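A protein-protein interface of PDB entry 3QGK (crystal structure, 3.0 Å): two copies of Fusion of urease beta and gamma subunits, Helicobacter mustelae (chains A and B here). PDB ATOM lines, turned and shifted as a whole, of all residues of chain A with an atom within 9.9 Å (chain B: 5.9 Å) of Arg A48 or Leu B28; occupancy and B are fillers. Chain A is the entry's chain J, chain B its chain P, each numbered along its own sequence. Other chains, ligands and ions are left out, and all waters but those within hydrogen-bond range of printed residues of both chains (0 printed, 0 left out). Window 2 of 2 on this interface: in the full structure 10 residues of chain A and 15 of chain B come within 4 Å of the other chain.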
ATOM      1  N   TYR A  14      11.742  -9.333  13.410  1.00  0.00           N
ATOM      2  CA  TYR A  14      10.621  -9.909  14.148  1.00  0.00           C
ATOM      3  C   TYR A  14      10.283  -9.121  15.403  1.00  0.00           C
ATOM      4  O   TYR A  14       9.099  -8.883  15.655  1.00  0.00           O
ATOM      5  CB  TYR A  14      10.801 -11.416  14.423  1.00  0.00           C
ATOM      6  CG  TYR A  14       9.498 -12.095  14.795  1.00  0.00           C
ATOM      7  CD1 TYR A  14       8.547 -12.405  13.826  1.00  0.00           C
ATOM      8  CD2 TYR A  14       9.185 -12.368  16.122  1.00  0.00           C
ATOM      9  CE1 TYR A  14       7.326 -12.980  14.169  1.00  0.00           C
ATOM     10  CE2 TYR A  14       7.976 -12.958  16.476  1.00  0.00           C
ATOM     11  CZ  TYR A  14       7.043 -13.257  15.498  1.00  0.00           C
ATOM     12  OH  TYR A  14       5.843 -13.824  15.874  1.00  0.00           O
ATOM     13  N   SER A  40       5.840  -7.725   7.823  1.00  0.00           N
ATOM     14  CA  SER A  40       6.942  -8.696   7.774  1.00  0.00           C
ATOM     15  C   SER A  40       6.781  -9.810   8.821  1.00  0.00           C
ATOM     16  O   SER A  40       6.881 -10.988   8.467  1.00  0.00           O
ATOM     17  CB  SER A  40       8.288  -8.003   7.926  1.00  0.00           C
ATOM     18  OG  SER A  40       8.475  -7.110   6.845  1.00  0.00           O
ATOM     19  N   ALA A  41       6.470  -9.441  10.082  1.00  0.00           N
ATOM     20  CA  ALA A  41       6.267 -10.390  11.166  1.00  0.00           C
ATOM     21  C   ALA A  41       5.090 -11.326  10.870  1.00  0.00           C
ATOM     22  O   ALA A  41       5.190 -12.521  11.155  1.00  0.00           O
ATOM     23  CB  ALA A  41       6.059  -9.654  12.475  1.00  0.00           C
ATOM     24  N   HIS A  42       4.000 -10.806  10.247  1.00  0.00           N
ATOM     25  CA  HIS A  42       2.846 -11.636   9.877  1.00  0.00           C
ATOM     26  C   HIS A  42       3.279 -12.705   8.875  1.00  0.00           C
ATOM     27  O   HIS A  42       2.939 -13.873   9.055  1.00  0.00           O
ATOM     28  CB  HIS A  42       1.684 -10.797   9.320  1.00  0.00           C
ATOM     29  CG  HIS A  42       0.603 -11.618   8.679  1.00  0.00           C
ATOM     30  ND1 HIS A  42      -0.267 -12.383   9.437  1.00  0.00           N
ATOM     31  CD2 HIS A  42       0.300 -11.786   7.366  1.00  0.00           C
ATOM     32  CE1 HIS A  42      -1.078 -12.976   8.569  1.00  0.00           C
ATOM     33  NE2 HIS A  42      -0.775 -12.649   7.310  1.00  0.00           N
ATOM     34  N   ILE A  43       4.051 -12.307   7.846  1.00  0.00           N
ATOM     35  CA  ILE A  43       4.559 -13.206   6.810  1.00  0.00           C
ATOM     36  C   ILE A  43       5.448 -14.284   7.430  1.00  0.00           C
ATOM     37  O   ILE A  43       5.254 -15.468   7.160  1.00  0.00           O
ATOM     38  CB  ILE A  43       5.231 -12.414   5.665  1.00  0.00           C
ATOM     39  CG1 ILE A  43       4.158 -11.641   4.856  1.00  0.00           C
ATOM     40  CG2 ILE A  43       6.035 -13.340   4.758  1.00  0.00           C
ATOM     41  CD1 ILE A  43       4.619 -10.425   4.088  1.00  0.00           C
ATOM     42  N   MET A  44       6.349 -13.878   8.330  1.00  0.00           N
ATOM     43  CA  MET A  44       7.255 -14.761   9.066  1.00  0.00           C
ATOM     44  C   MET A  44       6.501 -15.776   9.931  1.00  0.00           C
ATOM     45  O   MET A  44       6.949 -16.917  10.057  1.00  0.00           O
ATOM     46  CB  MET A  44       8.202 -13.926   9.930  1.00  0.00           C
ATOM     47  CG  MET A  44       9.267 -13.214   9.122  1.00  0.00           C
ATOM     48  SD  MET A  44      10.123 -11.947  10.063  1.00  0.00           S
ATOM     49  CE  MET A  44      11.420 -12.855  10.720  1.00  0.00           C
ATOM     50  N   ASP A  45       5.354 -15.359  10.509  1.00  0.00           N
ATOM     51  CA  ASP A  45       4.498 -16.196  11.349  1.00  0.00           C
ATOM     52  C   ASP A  45       3.812 -17.257  10.535  1.00  0.00           C
ATOM     53  O   ASP A  45       3.865 -18.426  10.912  1.00  0.00           O
ATOM     54  CB  ASP A  45       3.456 -15.354  12.099  1.00  0.00           C
ATOM     55  CG  ASP A  45       3.934 -14.799  13.426  1.00  0.00           C
ATOM     56  OD1 ASP A  45       4.960 -15.302  13.949  1.00  0.00           O
ATOM     57  OD2 ASP A  45       3.256 -13.895  13.970  1.00  0.00           O
ATOM     58  N   GLU A  46       3.174 -16.855   9.419  1.00  0.00           N
ATOM     59  CA  GLU A  46       2.439 -17.743   8.512  1.00  0.00           C
ATOM     60  C   GLU A  46       3.338 -18.792   7.851  1.00  0.00           C
ATOM     61  O   GLU A  46       2.910 -19.939   7.662  1.00  0.00           O
ATOM     62  CB  GLU A  46       1.664 -16.930   7.469  1.00  0.00           C
ATOM     63  CG  GLU A  46       0.475 -16.163   8.031  1.00  0.00           C
ATOM     64  CD  GLU A  46      -0.721 -16.951   8.549  1.00  0.00           C
ATOM     65  OE1 GLU A  46      -0.744 -18.197   8.413  1.00  0.00           O
ATOM     66  OE2 GLU A  46      -1.657 -16.308   9.077  1.00  0.00           O
ATOM     67  N   ALA A  47       4.589 -18.401   7.530  1.00  0.00           N
ATOM     68  CA  ALA A  47       5.605 -19.269   6.939  1.00  0.00           C
ATOM     69  C   ALA A  47       6.013 -20.372   7.918  1.00  0.00           C
ATOM     70  O   ALA A  47       6.234 -21.509   7.498  1.00  0.00           O
ATOM     71  CB  ALA A  47       6.817 -18.452   6.563  1.00  0.00           C
ATOM     72  N   ARG A  48       6.110 -20.039   9.220  1.00  0.00           N
ATOM     73  CA  ARG A  48       6.487 -20.994  10.263  1.00  0.00           C
ATOM     74  C   ARG A  48       5.384 -22.001  10.506  1.00  0.00           C
ATOM     75  O   ARG A  48       5.674 -23.174  10.761  1.00  0.00           O
ATOM     76  CB  ARG A  48       6.886 -20.286  11.569  1.00  0.00           C
ATOM     77  CG  ARG A  48       8.000 -20.994  12.320  1.00  0.00           C
ATOM     78  CD  ARG A  48       7.439 -22.066  13.204  1.00  0.00           C
ATOM     79  NE  ARG A  48       8.460 -22.924  13.795  1.00  0.00           N
ATOM     80  CZ  ARG A  48       8.294 -24.225  14.022  1.00  0.00           C
ATOM     81  NH1 ARG A  48       7.174 -24.837  13.644  1.00  0.00           N
ATOM     82  NH2 ARG A  48       9.253 -24.927  14.606  1.00  0.00           N
ATOM     83  N   ARG A  49       4.123 -21.554  10.395  1.00  0.00           N
ATOM     84  CA  ARG A  49       2.941 -22.403  10.539  1.00  0.00           C
ATOM     85  C   ARG A  49       2.866 -23.424   9.379  1.00  0.00           C
ATOM     86  O   ARG A  49       2.266 -24.487   9.541  1.00  0.00           O
ATOM     87  CB  ARG A  49       1.677 -21.543  10.616  1.00  0.00           C
ATOM     88  CG  ARG A  49       1.594 -20.748  11.898  1.00  0.00           C
ATOM     89  CD  ARG A  49       0.415 -19.800  11.918  1.00  0.00           C
ATOM     90  NE  ARG A  49       0.487 -18.885  13.059  1.00  0.00           N
ATOM     91  CZ  ARG A  49       0.309 -17.570  12.977  1.00  0.00           C
ATOM     92  NH1 ARG A  49       0.018 -17.003  11.812  1.00  0.00           N
ATOM     93  NH2 ARG A  49       0.409 -16.812  14.063  1.00  0.00           N
ATOM     94  N   GLY A  50       3.516 -23.085   8.254  1.00  0.00           N
ATOM     95  CA  GLY A  50       3.657 -23.902   7.054  1.00  0.00           C
ATOM     96  C   GLY A  50       2.373 -24.466   6.499  1.00  0.00           C
ATOM     97  O   GLY A  50       2.331 -25.632   6.095  1.00  0.00           O
ATOM     98  N   LYS A  51       1.317 -23.642   6.498  1.00  0.00           N
ATOM     99  CA  LYS A  51      -0.002 -24.037   5.993  1.00  0.00           C
ATOM    100  C   LYS A  51      -0.424 -23.214   4.771  1.00  0.00           C
ATOM    101  O   LYS A  51      -1.341 -23.607   4.052  1.00  0.00           O
ATOM    102  CB  LYS A  51      -1.056 -23.969   7.109  1.00  0.00           C
ATOM    103  CG  LYS A  51      -1.457 -25.340   7.617  1.00  0.00           C
ATOM    104  CD  LYS A  51      -1.206 -25.511   9.111  1.00  0.00           C
ATOM    105  CE  LYS A  51      -1.218 -26.969   9.530  1.00  0.00           C
ATOM    106  NZ  LYS A  51      -0.016 -27.714   9.046  1.00  0.00           N
ATOM    107  N   LYS A  52       0.260 -22.085   4.529  1.00  0.00           N
ATOM    108  CA  LYS A  52      -0.035 -21.220   3.395  1.00  0.00           C
ATOM    109  C   LYS A  52       1.093 -21.213   2.379  1.00  0.00           C
ATOM    110  O   LYS A  52       2.275 -21.329   2.744  1.00  0.00           O
ATOM    111  CB  LYS A  52      -0.351 -19.799   3.861  1.00  0.00           C
ATOM    112  CG  LYS A  52      -1.705 -19.676   4.538  1.00  0.00           C
ATOM    113  CD  LYS A  52      -1.886 -18.306   5.114  1.00  0.00           C
ATOM    114  CE  LYS A  52      -3.145 -18.226   5.917  1.00  0.00           C
ATOM    115  NZ  LYS A  52      -3.298 -16.887   6.535  1.00  0.00           N
ATOM    116  N   THR A  53       0.719 -21.102   1.093  1.00  0.00           N
ATOM    117  CA  THR A  53       1.682 -21.047   0.000  1.00  0.00           C
ATOM    118  C   THR A  53       2.163 -19.621  -0.171  1.00  0.00           C
ATOM    119  O   THR A  53       1.539 -18.694   0.358  1.00  0.00           O
ATOM    120  CB  THR A  53       1.088 -21.607  -1.299  1.00  0.00           C
ATOM    121  OG1 THR A  53      -0.036 -20.835  -1.705  1.00  0.00           O
ATOM    122  CG2 THR A  53       0.717 -23.070  -1.191  1.00  0.00           C
ATOM    123  N   LEU A  57      -0.025 -15.984   0.391  1.00  0.00           N
ATOM    124  CA  LEU A  57       0.465 -14.852   1.174  1.00  0.00           C
ATOM    125  C   LEU A  57       0.594 -13.563   0.378  1.00  0.00           C
ATOM    126  O   LEU A  57       0.230 -12.502   0.887  1.00  0.00           O
ATOM    127  CB  LEU A  57       1.783 -15.202   1.876  1.00  0.00           C
ATOM    128  CG  LEU A  57       1.681 -16.215   3.013  1.00  0.00           C
ATOM    129  CD1 LEU A  57       3.060 -16.614   3.513  1.00  0.00           C
ATOM    130  CD2 LEU A  57       0.846 -15.673   4.159  1.00  0.00           C
ATOM    131  N   GLU A  84      11.900 -12.664   2.963  1.00  0.00           N
ATOM    132  CA  GLU A  84      12.332 -14.047   2.816  1.00  0.00           C
ATOM    133  C   GLU A  84      12.028 -14.764   4.115  1.00  0.00           C
ATOM    134  O   GLU A  84      12.345 -14.258   5.193  1.00  0.00           O
ATOM    135  CB  GLU A  84      13.835 -14.110   2.553  1.00  0.00           C
ATOM    136  CG  GLU A  84      14.245 -13.579   1.194  1.00  0.00           C
ATOM    137  CD  GLU A  84      15.078 -14.533   0.364  1.00  0.00           C
ATOM    138  OE1 GLU A  84      15.943 -15.241   0.936  1.00  0.00           O
ATOM    139  OE2 GLU A  84      14.904 -14.523  -0.878  1.00  0.00           O
ATOM    140  N   ALA A  85      11.399 -15.929   4.026  1.00  0.00           N
ATOM    141  CA  ALA A  85      11.060 -16.708   5.217  1.00  0.00           C
ATOM    142  C   ALA A  85      11.199 -18.201   4.960  1.00  0.00           C
ATOM    143  O   ALA A  85      11.077 -18.627   3.810  1.00  0.00           O
ATOM    144  CB  ALA A  85       9.647 -16.381   5.665  1.00  0.00           C
ATOM    145  N   ASN A  86      11.466 -18.994   6.016  1.00  0.00           N
ATOM    146  CA  ASN A  86      11.573 -20.436   5.854  1.00  0.00           C
ATOM    147  C   ASN A  86      10.202 -21.079   5.897  1.00  0.00           C
ATOM    148  O   ASN A  86       9.453 -20.927   6.873  1.00  0.00           O
ATOM    149  CB  ASN A  86      12.530 -21.100   6.853  1.00  0.00           C
ATOM    150  CG  ASN A  86      12.736 -22.586   6.591  1.00  0.00           C
ATOM    151  OD1 ASN A  86      13.562 -22.985   5.764  1.00  0.00           O
ATOM    152  ND2 ASN A  86      11.999 -23.440   7.286  1.00  0.00           N
ATOM    153  N   PHE A  87       9.890 -21.795   4.812  1.00  0.00           N
ATOM    154  CA  PHE A  87       8.675 -22.573   4.600  1.00  0.00           C
ATOM    155  C   PHE A  87       9.082 -24.056   4.731  1.00  0.00           C
ATOM    156  O   PHE A  87      10.290 -24.326   4.749  1.00  0.00           O
ATOM    157  CB  PHE A  87       8.143 -22.293   3.190  1.00  0.00           C
ATOM    158  CG  PHE A  87       7.475 -20.954   3.027  1.00  0.00           C
ATOM    159  CD1 PHE A  87       8.217 -19.823   2.716  1.00  0.00           C
ATOM    160  CD2 PHE A  87       6.099 -20.827   3.148  1.00  0.00           C
ATOM    161  CE1 PHE A  87       7.597 -18.584   2.551  1.00  0.00           C
ATOM    162  CE2 PHE A  87       5.477 -19.584   2.979  1.00  0.00           C
ATOM    163  CZ  PHE A  87       6.230 -18.473   2.677  1.00  0.00           C
ATOM    164  N   PRO A  88       8.138 -25.039   4.801  1.00  0.00           N
ATOM    165  CA  PRO A  88       8.560 -26.455   4.920  1.00  0.00           C
ATOM    166  C   PRO A  88       9.432 -26.937   3.761  1.00  0.00           C
ATOM    167  O   PRO A  88      10.250 -27.834   3.947  1.00  0.00           O
ATOM    168  CB  PRO A  88       7.236 -27.210   5.000  1.00  0.00           C
ATOM    169  CG  PRO A  88       6.251 -26.197   5.490  1.00  0.00           C
ATOM    170  CD  PRO A  88       6.665 -24.926   4.834  1.00  0.00           C
ATOM    171  N   ASP A  89       9.296 -26.284   2.595  1.00  0.00           N
ATOM    172  CA  ASP A  89      10.056 -26.537   1.367  1.00  0.00           C
ATOM    173  C   ASP A  89      11.306 -25.627   1.226  1.00  0.00           C
ATOM    174  O   ASP A  89      11.921 -25.592   0.157  1.00  0.00           O
ATOM    175  CB  ASP A  89       9.139 -26.403   0.132  1.00  0.00           C
ATOM    176  CG  ASP A  89       8.431 -25.065   0.009  1.00  0.00           C
ATOM    177  OD1 ASP A  89       7.773 -24.650   0.986  1.00  0.00           O
ATOM    178  OD2 ASP A  89       8.492 -24.460  -1.079  1.00  0.00           O
ATOM    179  N   GLY A  90      11.688 -24.938   2.303  1.00  0.00           N
ATOM    180  CA  GLY A  90      12.853 -24.056   2.319  1.00  0.00           C
ATOM    181  C   GLY A  90      12.557 -22.561   2.317  1.00  0.00           C
ATOM    182  O   GLY A  90      11.385 -22.158   2.322  1.00  0.00           O
ATOM    183  N   VAL A  94       8.638 -13.843  -0.260  1.00  0.00           N
ATOM    184  CA  VAL A  94       7.252 -13.374  -0.301  1.00  0.00           C
ATOM    185  C   VAL A  94       7.279 -11.914  -0.761  1.00  0.00           C
ATOM    186  O   VAL A  94       7.852 -11.060  -0.078  1.00  0.00           O
ATOM    187  CB  VAL A  94       6.516 -13.577   1.047  1.00  0.00           C
ATOM    188  CG1 VAL A  94       5.077 -13.077   0.978  1.00  0.00           C
ATOM    189  CG2 VAL A  94       6.545 -15.043   1.460  1.00  0.00           C
ATOM    190  N   ARG B  23       5.648 -19.785  20.038  1.00  0.00           N
ATOM    191  CA  ARG B  23       5.420 -20.838  19.047  1.00  0.00           C
ATOM    192  C   ARG B  23       4.888 -22.142  19.665  1.00  0.00           C
ATOM    193  O   ARG B  23       4.018 -22.780  19.072  1.00  0.00           O
ATOM    194  CB  ARG B  23       6.686 -21.061  18.205  1.00  0.00           C
ATOM    195  CG  ARG B  23       6.988 -19.857  17.328  1.00  0.00           C
ATOM    196  CD  ARG B  23       8.257 -19.959  16.520  1.00  0.00           C
ATOM    197  NE  ARG B  23       8.237 -18.975  15.437  1.00  0.00           N
ATOM    198  CZ  ARG B  23       9.236 -18.758  14.586  1.00  0.00           C
ATOM    199  NH1 ARG B  23      10.368 -19.447  14.687  1.00  0.00           N
ATOM    200  NH2 ARG B  23       9.105 -17.865  13.612  1.00  0.00           N
ATOM    201  N   LYS B  24       5.381 -22.513  20.869  1.00  0.00           N
ATOM    202  CA  LYS B  24       4.919 -23.688  21.618  1.00  0.00           C
ATOM    203  C   LYS B  24       3.460 -23.452  22.055  1.00  0.00           C
ATOM    204  O   LYS B  24       2.637 -24.366  21.957  1.00  0.00           O
ATOM    205  CB  LYS B  24       5.814 -23.940  22.842  1.00  0.00           C
ATOM    206  CG  LYS B  24       5.549 -25.276  23.535  1.00  0.00           C
ATOM    207  CD  LYS B  24       6.537 -25.545  24.658  1.00  0.00           C
ATOM    208  CE  LYS B  24       6.147 -26.702  25.538  1.00  0.00           C
ATOM    209  NZ  LYS B  24       5.166 -26.298  26.582  1.00  0.00           N
ATOM    210  N   GLU B  25       3.139 -22.211  22.502  1.00  0.00           N
ATOM    211  CA  GLU B  25       1.789 -21.793  22.907  1.00  0.00           C
ATOM    212  C   GLU B  25       0.825 -21.878  21.721  1.00  0.00           C
ATOM    213  O   GLU B  25      -0.336 -22.220  21.919  1.00  0.00           O
ATOM    214  CB  GLU B  25       1.795 -20.385  23.524  1.00  0.00           C
ATOM    215  CG  GLU B  25       2.339 -20.342  24.948  1.00  0.00           C
ATOM    216  CD  GLU B  25       2.948 -19.026  25.417  1.00  0.00           C
ATOM    217  OE1 GLU B  25       2.333 -17.959  25.188  1.00  0.00           O
ATOM    218  OE2 GLU B  25       4.024 -19.069  26.058  1.00  0.00           O
ATOM    219  N   GLU B  26       1.325 -21.626  20.489  1.00  0.00           N
ATOM    220  CA  GLU B  26       0.576 -21.741  19.228  1.00  0.00           C
ATOM    221  C   GLU B  26       0.343 -23.224  18.869  1.00  0.00           C
ATOM    222  O   GLU B  26      -0.413 -23.518  17.936  1.00  0.00           O
ATOM    223  CB  GLU B  26       1.337 -21.075  18.066  1.00  0.00           C
ATOM    224  CG  GLU B  26       1.213 -19.565  17.988  1.00  0.00           C
ATOM    225  CD  GLU B  26       1.981 -18.924  16.844  1.00  0.00           C
ATOM    226  OE1 GLU B  26       1.896 -19.435  15.702  1.00  0.00           O
ATOM    227  OE2 GLU B  26       2.642 -17.887  17.084  1.00  0.00           O
ATOM    228  N   GLY B  27       1.024 -24.131  19.575  1.00  0.00           N
ATOM    229  CA  GLY B  27       0.916 -25.566  19.358  1.00  0.00           C
ATOM    230  C   GLY B  27       1.874 -26.112  18.326  1.00  0.00           C
ATOM    231  O   GLY B  27       1.662 -27.212  17.813  1.00  0.00           O
ATOM    232  N   LEU B  28       2.940 -25.366  18.012  1.00  0.00           N
ATOM    233  CA  LEU B  28       3.935 -25.828  17.048  1.00  0.00           C
ATOM    234  C   LEU B  28       5.004 -26.676  17.739  1.00  0.00           C
ATOM    235  O   LEU B  28       5.424 -26.372  18.862  1.00  0.00           O
ATOM    236  CB  LEU B  28       4.606 -24.639  16.335  1.00  0.00           C
ATOM    237  CG  LEU B  28       3.723 -23.673  15.544  1.00  0.00           C
ATOM    238  CD1 LEU B  28       4.353 -22.309  15.494  1.00  0.00           C
ATOM    239  CD2 LEU B  28       3.520 -24.142  14.133  1.00  0.00           C
ATOM    240  N   LYS B  29       5.451 -27.736  17.058  1.00  0.00           N
ATOM    241  CA  LYS B  29       6.546 -28.588  17.525  1.00  0.00           C
ATOM    242  C   LYS B  29       7.843 -27.800  17.256  1.00  0.00           C
ATOM    243  O   LYS B  29       8.099 -27.384  16.112  1.00  0.00           O
ATOM    244  CB  LYS B  29       6.571 -29.928  16.778  1.00  0.00           C
ATOM    245  CG  LYS B  29       5.512 -30.909  17.243  1.00  0.00           C
ATOM    246  CD  LYS B  29       5.680 -32.220  16.509  1.00  0.00           C
ATOM    247  CE  LYS B  29       4.703 -33.277  16.923  1.00  0.00           C
ATOM    248  NZ  LYS B  29       5.097 -34.588  16.344  1.00  0.00           N
ATOM    249  N   LEU B  30       8.610 -27.535  18.325  1.00  0.00           N
ATOM    250  CA  LEU B  30       9.839 -26.761  18.253  1.00  0.00           C
ATOM    251  C   LEU B  30      10.971 -27.480  17.503  1.00  0.00           C
ATOM    252  O   LEU B  30      11.067 -28.707  17.556  1.00  0.00           O
ATOM    253  CB  LEU B  30      10.296 -26.343  19.659  1.00  0.00           C
ATOM    254  CG  LEU B  30       9.315 -25.540  20.528  1.00  0.00           C
ATOM    255  CD1 LEU B  30       9.918 -25.244  21.876  1.00  0.00           C
ATOM    256  CD2 LEU B  30       8.889 -24.242  19.863  1.00  0.00           C
ATOM    257  N   ASN B  31      11.814 -26.714  16.784  1.00  0.00           N
ATOM    258  CA  ASN B  31      12.960 -27.260  16.049  1.00  0.00           C
ATOM    259  C   ASN B  31      14.217 -27.185  16.929  1.00  0.00           C
ATOM    260  O   ASN B  31      14.098 -26.771  18.088  1.00  0.00           O
ATOM    261  CB  ASN B  31      13.150 -26.545  14.703  1.00  0.00           C
ATOM    262  CG  ASN B  31      13.272 -25.041  14.760  1.00  0.00           C
ATOM    263  OD1 ASN B  31      13.909 -24.467  15.644  1.00  0.00           O
ATOM    264  ND2 ASN B  31      12.691 -24.368  13.778  1.00  0.00           N
ATOM    265  N   GLU B  34      15.030 -23.504  18.409  1.00  0.00           N
ATOM    266  CA  GLU B  34      13.887 -23.101  19.234  1.00  0.00           C
ATOM    267  C   GLU B  34      13.917 -23.843  20.566  1.00  0.00           C
ATOM    268  O   GLU B  34      13.801 -23.201  21.612  1.00  0.00           O
ATOM    269  CB  GLU B  34      12.560 -23.345  18.508  1.00  0.00           C
ATOM    270  CG  GLU B  34      12.271 -22.376  17.371  1.00  0.00           C
ATOM    271  CD  GLU B  34      11.124 -22.766  16.452  1.00  0.00           C
ATOM    272  OE1 GLU B  34      10.580 -23.883  16.610  1.00  0.00           O
ATOM    273  OE2 GLU B  34      10.770 -21.956  15.565  1.00  0.00           O
ATOM    274  N   GLU B  69       6.747 -32.560  21.897  1.00  0.00           N
ATOM    275  CA  GLU B  69       6.739 -31.096  22.039  1.00  0.00           C
ATOM    276  C   GLU B  69       7.737 -30.473  21.047  1.00  0.00           C
ATOM    277  O   GLU B  69       7.717 -29.255  20.816  1.00  0.00           O
ATOM    278  CB  GLU B  69       7.072 -30.668  23.491  1.00  0.00           C
ATOM    279  CG  GLU B  69       6.094 -31.144  24.559  1.00  0.00           C
ATOM    280  CD  GLU B  69       6.307 -30.567  25.947  1.00  0.00           C
ATOM    281  OE1 GLU B  69       7.379 -30.806  26.551  1.00  0.00           O
ATOM    282  OE2 GLU B  69       5.378 -29.894  26.446  1.00  0.00           O
ATOM    283  N   MET B  71      10.118 -31.354  17.118  1.00  0.00           N
ATOM    284  CA  MET B  71      10.139 -32.041  15.825  1.00  0.00           C
ATOM    285  C   MET B  71      10.932 -33.360  15.962  1.00  0.00           C
ATOM    286  O   MET B  71      11.728 -33.483  16.897  1.00  0.00           O
ATOM    287  CB  MET B  71      10.830 -31.158  14.773  1.00  0.00           C
ATOM    288  CG  MET B  71      10.038 -29.957  14.367  1.00  0.00           C
ATOM    289  SD  MET B  71      10.931 -29.043  13.096  1.00  0.00           S
ATOM    290  CE  MET B  71       9.840 -27.696  12.862  1.00  0.00           C
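CG of Arg A48 touches CZ of Arg B23, at 3.4 Å. CB of Leu B28 touches NH1 of Arg A48 (3.7 Å). Asn B31 touches Arg A48. Met B71 touches Arg A48.
Of the 24 printed residues of chain A, 2 touch a printed residue of chain B. Among the printed residues, 7 pairs touch across the chains. Among the printed residues, Asp or Glu carboxylates within 4 Å of a Lys or Arg side-chain nitrogen of the other chain: Arg A48 with Glu B34 and Arg A49 with Glu B26.
Of chain B, only Arg B23 (3.4 Å), Leu B28 (3.7 Å), Lys B29 (3.1 Å), Asn B31 (3.6 Å), Glu B34 (2.6 Å) and Met B71 (3.3 Å) come within 4 Å of Arg A48. Of chain A, only Arg A48 comes within 4 Å of Leu B28. Arg B23 touches just one residue of chain A: Arg A48. Printed residues of chain A within 4 Å of Glu B34: Arg A48 (2.6 Å). Printed residues of chain A within 4 Å of Asn B31: Arg A48. The nearest residue of chain A that does not touch Leu B28 is Arg A49 (4.03 Å). The nearest printed residue of chain A that does not touch Glu B34 is Met A44 (8.4 Å).
No position is printed for both chains.
OE1 of Glu B34 lies within salt-bridge range of NH2 of Arg A48. The guanidinium group (NE) of Arg A49 lies within salt-bridge range of the side-chain carboxylate (OE1) of Glu B26 (3.0 Å). The guanidinium group (NH2) of Arg A48 sits at hydrogen-bond distance from the backbone carbonyl oxygen (O) of Lys B29 (3.1 Å).
The side-chain carboxylate (OE2) of Glu A46 lies within salt-bridge range of the guanidinium group (NH1) of Arg A49. The guanidinium group of Arg B23 is in salt-bridge range of the side-chain carboxylate of Glu B34, at 2.7 Å. O of Leu B30 is in hydrogen-bond range of N of Met B71 (2.8 Å). The backbone NH (N) of Leu B28 lies within hydrogen-bond range of the backbone carbonyl oxygen (O) of Arg B23, 3.0 Å away. The backbone NH (N) of Asn B31 is in hydrogen-bond range of the side-chain carboxylate (OE1) of Glu B34.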
